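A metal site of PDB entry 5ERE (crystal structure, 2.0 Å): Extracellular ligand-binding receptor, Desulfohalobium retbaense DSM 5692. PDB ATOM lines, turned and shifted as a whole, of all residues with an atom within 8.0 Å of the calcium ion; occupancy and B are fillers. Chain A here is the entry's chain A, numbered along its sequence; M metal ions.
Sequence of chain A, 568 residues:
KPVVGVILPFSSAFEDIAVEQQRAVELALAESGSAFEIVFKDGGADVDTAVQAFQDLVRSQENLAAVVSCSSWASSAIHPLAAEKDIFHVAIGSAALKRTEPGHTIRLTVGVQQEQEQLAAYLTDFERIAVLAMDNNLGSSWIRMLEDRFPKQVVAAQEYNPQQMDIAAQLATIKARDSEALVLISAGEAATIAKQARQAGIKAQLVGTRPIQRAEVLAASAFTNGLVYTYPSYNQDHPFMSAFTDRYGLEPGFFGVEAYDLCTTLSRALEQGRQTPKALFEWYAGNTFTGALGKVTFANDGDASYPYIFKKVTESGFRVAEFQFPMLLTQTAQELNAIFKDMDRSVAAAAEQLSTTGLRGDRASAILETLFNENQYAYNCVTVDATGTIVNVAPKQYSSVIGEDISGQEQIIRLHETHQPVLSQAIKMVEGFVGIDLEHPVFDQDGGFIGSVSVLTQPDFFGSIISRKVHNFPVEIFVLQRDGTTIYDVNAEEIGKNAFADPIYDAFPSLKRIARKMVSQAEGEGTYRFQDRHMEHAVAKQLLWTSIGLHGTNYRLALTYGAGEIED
The side-chain amide oxygen of Asn 287 sits close to the backbone carbonyl oxygen of Trp 283, at 3.3 Å. N of Phe 298 lies within hydrogen-bond range of O of Asn 287, at 2.7 Å.
The calcium ion is bound by the backbone carbonyl oxygen of Glu 282, the side-chain amide oxygen of Asn 287, the side-chain carboxylate of Glu 282 and the backbone carbonyl oxygen of Ala 285. The calcium ion has four donor atoms within binding distance.
Of the 15 residues printed, 3 come within 4 Å of the calcium ion. The nearest printed residue that does not touch the calcium ion is Trp 283 (4.2 Å).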
ATOM      1  N   LYS A 278      13.783  23.614 -19.260  1.00  0.00           N
ATOM      2  CA  LYS A 278      13.831  24.912 -19.884  1.00  0.00           C
ATOM      3  C   LYS A 278      15.261  25.267 -20.274  1.00  0.00           C
ATOM      4  O   LYS A 278      15.493  25.858 -21.328  1.00  0.00           O
ATOM      5  CB  LYS A 278      13.286  25.997 -18.951  1.00  0.00           C
ATOM      6  CG  LYS A 278      11.766  26.085 -18.902  1.00  0.00           C
ATOM      7  CD  LYS A 278      11.267  27.498 -18.516  1.00  0.00           C
ATOM      8  CE  LYS A 278      11.451  28.508 -19.657  1.00  0.00           C
ATOM      9  NZ  LYS A 278      10.532  29.689 -19.530  1.00  0.00           N
ATOM     10  N   ALA A 279      16.215  24.963 -19.419  1.00  0.00           N
ATOM     11  CA  ALA A 279      17.599  25.355 -19.714  1.00  0.00           C
ATOM     12  C   ALA A 279      18.141  24.491 -20.852  1.00  0.00           C
ATOM     13  O   ALA A 279      18.883  24.948 -21.718  1.00  0.00           O
ATOM     14  CB  ALA A 279      18.468  25.220 -18.474  1.00  0.00           C
ATOM     15  N   LEU A 280      17.745  23.230 -20.855  1.00  0.00           N
ATOM     16  CA  LEU A 280      18.225  22.300 -21.867  1.00  0.00           C
ATOM     17  C   LEU A 280      17.630  22.646 -23.217  1.00  0.00           C
ATOM     18  O   LEU A 280      18.324  22.596 -24.230  1.00  0.00           O
ATOM     19  CB  LEU A 280      17.921  20.873 -21.443  1.00  0.00           C
ATOM     20  CG  LEU A 280      18.919  20.354 -20.423  1.00  0.00           C
ATOM     21  CD1 LEU A 280      18.449  19.089 -19.796  1.00  0.00           C
ATOM     22  CD2 LEU A 280      20.278  20.145 -21.045  1.00  0.00           C
ATOM     23  N   PHE A 281      16.340  22.989 -23.241  1.00  0.00           N
ATOM     24  CA  PHE A 281      15.694  23.441 -24.461  1.00  0.00           C
ATOM     25  C   PHE A 281      16.372  24.716 -25.002  1.00  0.00           C
ATOM     26  O   PHE A 281      16.736  24.793 -26.183  1.00  0.00           O
ATOM     27  CB  PHE A 281      14.190  23.644 -24.208  1.00  0.00           C
ATOM     28  CG  PHE A 281      13.358  23.853 -25.452  1.00  0.00           C
ATOM     29  CD1 PHE A 281      13.298  25.094 -26.065  1.00  0.00           C
ATOM     30  CD2 PHE A 281      12.591  22.817 -25.978  1.00  0.00           C
ATOM     31  CE1 PHE A 281      12.531  25.286 -27.189  1.00  0.00           C
ATOM     32  CE2 PHE A 281      11.815  22.995 -27.103  1.00  0.00           C
ATOM     33  CZ  PHE A 281      11.776  24.223 -27.717  1.00  0.00           C
ATOM     34  N   GLU A 282      16.616  25.701 -24.130  1.00  0.00           N
ATOM     35  CA  GLU A 282      17.240  26.948 -24.562  1.00  0.00           C
ATOM     36  C   GLU A 282      18.684  26.753 -25.072  1.00  0.00           C
ATOM     37  O   GLU A 282      19.190  27.502 -25.923  1.00  0.00           O
ATOM     38  CB  GLU A 282      17.221  27.983 -23.416  1.00  0.00           C
ATOM     39  CG  GLU A 282      17.879  29.313 -23.810  1.00  0.00           C
ATOM     40  CD  GLU A 282      17.168  30.004 -24.972  1.00  0.00           C
ATOM     41  OE1 GLU A 282      15.955  30.274 -24.801  1.00  0.00           O
ATOM     42  OE2 GLU A 282      17.791  30.242 -26.056  1.00  0.00           O
ATOM     43  N   TRP A 283      19.345  25.752 -24.527  1.00  0.00           N
ATOM     44  CA  TRP A 283      20.667  25.386 -25.025  1.00  0.00           C
ATOM     45  C   TRP A 283      20.648  25.190 -26.532  1.00  0.00           C
ATOM     46  O   TRP A 283      21.599  25.558 -27.244  1.00  0.00           O
ATOM     47  CB  TRP A 283      21.118  24.098 -24.368  1.00  0.00           C
ATOM     48  CG  TRP A 283      22.459  23.696 -24.783  1.00  0.00           C
ATOM     49  CD1 TRP A 283      22.773  22.872 -25.818  1.00  0.00           C
ATOM     50  CD2 TRP A 283      23.685  24.139 -24.203  1.00  0.00           C
ATOM     51  NE1 TRP A 283      24.146  22.753 -25.917  1.00  0.00           N
ATOM     52  CE2 TRP A 283      24.729  23.519 -24.943  1.00  0.00           C
ATOM     53  CE3 TRP A 283      24.020  24.982 -23.143  1.00  0.00           C
ATOM     54  CZ2 TRP A 283      26.049  23.718 -24.634  1.00  0.00           C
ATOM     55  CZ3 TRP A 283      25.350  25.174 -22.828  1.00  0.00           C
ATOM     56  CH2 TRP A 283      26.345  24.545 -23.577  1.00  0.00           C
ATOM     57  N   TYR A 284      19.587  24.560 -27.012  1.00  0.00           N
ATOM     58  CA  TYR A 284      19.480  24.251 -28.435  1.00  0.00           C
ATOM     59  C   TYR A 284      18.743  25.335 -29.208  1.00  0.00           C
ATOM     60  O   TYR A 284      19.187  25.733 -30.283  1.00  0.00           O
ATOM     61  CB  TYR A 284      18.795  22.891 -28.600  1.00  0.00           C
ATOM     62  CG  TYR A 284      19.693  21.722 -28.235  1.00  0.00           C
ATOM     63  CD1 TYR A 284      20.608  21.218 -29.145  1.00  0.00           C
ATOM     64  CD2 TYR A 284      19.576  21.106 -27.009  1.00  0.00           C
ATOM     65  CE1 TYR A 284      21.441  20.156 -28.807  1.00  0.00           C
ATOM     66  CE2 TYR A 284      20.368  20.054 -26.657  1.00  0.00           C
ATOM     67  CZ  TYR A 284      21.301  19.579 -27.563  1.00  0.00           C
ATOM     68  OH  TYR A 284      22.052  18.508 -27.186  1.00  0.00           O
ATOM     69  N   ALA A 285      17.632  25.843 -28.654  1.00  0.00           N
ATOM     70  CA  ALA A 285      16.725  26.707 -29.392  1.00  0.00           C
ATOM     71  C   ALA A 285      17.439  27.982 -29.839  1.00  0.00           C
ATOM     72  O   ALA A 285      17.999  28.704 -29.012  1.00  0.00           O
ATOM     73  CB  ALA A 285      15.469  27.052 -28.510  1.00  0.00           C
ATOM     74  N   GLY A 286      17.385  28.275 -31.141  1.00  0.00           N
ATOM     75  CA  GLY A 286      18.030  29.439 -31.723  1.00  0.00           C
ATOM     76  C   GLY A 286      19.514  29.275 -32.023  1.00  0.00           C
ATOM     77  O   GLY A 286      20.149  30.189 -32.546  1.00  0.00           O
ATOM     78  N   ASN A 287      20.072  28.119 -31.697  1.00  0.00           N
ATOM     79  CA  ASN A 287      21.516  27.966 -31.776  1.00  0.00           C
ATOM     80  C   ASN A 287      21.933  27.263 -33.030  1.00  0.00           C
ATOM     81  O   ASN A 287      21.155  26.520 -33.639  1.00  0.00           O
ATOM     82  CB  ASN A 287      22.087  27.218 -30.554  1.00  0.00           C
ATOM     83  CG  ASN A 287      22.143  28.078 -29.324  1.00  0.00           C
ATOM     84  OD1 ASN A 287      21.110  28.474 -28.814  1.00  0.00           O
ATOM     85  ND2 ASN A 287      23.372  28.362 -28.846  1.00  0.00           N
ATOM     86  N   THR A 288      23.187  27.503 -33.367  1.00  0.00           N
ATOM     87  CA  THR A 288      23.837  26.856 -34.479  1.00  0.00           C
ATOM     88  C   THR A 288      24.942  25.970 -33.913  1.00  0.00           C
ATOM     89  O   THR A 288      25.666  26.388 -33.005  1.00  0.00           O
ATOM     90  CB  THR A 288      24.383  27.904 -35.453  1.00  0.00           C
ATOM     91  OG1 THR A 288      23.262  28.641 -35.963  1.00  0.00           O
ATOM     92  CG2 THR A 288      25.165  27.232 -36.598  1.00  0.00           C
ATOM     93  N   PHE A 289      25.005  24.734 -34.388  1.00  0.00           N
ATOM     94  CA  PHE A 289      26.101  23.820 -34.047  1.00  0.00           C
ATOM     95  C   PHE A 289      26.703  23.219 -35.291  1.00  0.00           C
ATOM     96  O   PHE A 289      25.978  22.886 -36.254  1.00  0.00           O
ATOM     97  CB  PHE A 289      25.604  22.678 -33.173  1.00  0.00           C
ATOM     98  CG  PHE A 289      24.989  23.110 -31.883  1.00  0.00           C
ATOM     99  CD1 PHE A 289      23.638  23.396 -31.801  1.00  0.00           C
ATOM    100  CD2 PHE A 289      25.769  23.229 -30.741  1.00  0.00           C
ATOM    101  CE1 PHE A 289      23.068  23.798 -30.612  1.00  0.00           C
ATOM    102  CE2 PHE A 289      25.207  23.651 -29.529  1.00  0.00           C
ATOM    103  CZ  PHE A 289      23.847  23.931 -29.469  1.00  0.00           C
ATOM    104  N   PHE A 298      19.037  25.543 -35.059  1.00  0.00           N
ATOM    105  CA  PHE A 298      17.737  25.239 -34.468  1.00  0.00           C
ATOM    106  C   PHE A 298      16.848  26.487 -34.418  1.00  0.00           C
ATOM    107  O   PHE A 298      17.265  27.560 -33.965  1.00  0.00           O
ATOM    108  CB  PHE A 298      17.891  24.664 -33.071  1.00  0.00           C
ATOM    109  CG  PHE A 298      18.510  23.310 -33.005  1.00  0.00           C
ATOM    110  CD1 PHE A 298      19.882  23.180 -33.071  1.00  0.00           C
ATOM    111  CD2 PHE A 298      17.740  22.168 -32.838  1.00  0.00           C
ATOM    112  CE1 PHE A 298      20.503  21.953 -32.978  1.00  0.00           C
ATOM    113  CE2 PHE A 298      18.352  20.925 -32.733  1.00  0.00           C
ATOM    114  CZ  PHE A 298      19.762  20.825 -32.794  1.00  0.00           C
ATOM    115  N   ALA A 299      15.601  26.334 -34.862  1.00  0.00           N
ATOM    116  CA  ALA A 299      14.601  27.395 -34.786  1.00  0.00           C
ATOM    117  C   ALA A 299      14.221  27.617 -33.332  1.00  0.00           C
ATOM    118  O   ALA A 299      14.541  26.773 -32.491  1.00  0.00           O
ATOM    119  CB  ALA A 299      13.321  27.025 -35.623  1.00  0.00           C
ATOM    120  N   ASN A 300      13.511  28.717 -33.058  1.00  0.00           N
ATOM    121  CA  ASN A 300      12.954  28.955 -31.722  1.00  0.00           C
ATOM    122  C   ASN A 300      12.031  27.820 -31.225  1.00  0.00           C
ATOM    123  O   ASN A 300      11.964  27.603 -30.033  1.00  0.00           O
ATOM    124  CB  ASN A 300      12.162  30.281 -31.690  1.00  0.00           C
ATOM    125  CG  ASN A 300      13.055  31.518 -31.807  1.00  0.00           C
ATOM    126  OD1 ASN A 300      14.289  31.421 -31.718  1.00  0.00           O
ATOM    127  ND2 ASN A 300      12.431  32.684 -31.992  1.00  0.00           N
HETATM  128 CA    CA M   1      19.554  29.269 -27.277  1.00  0.00          CA
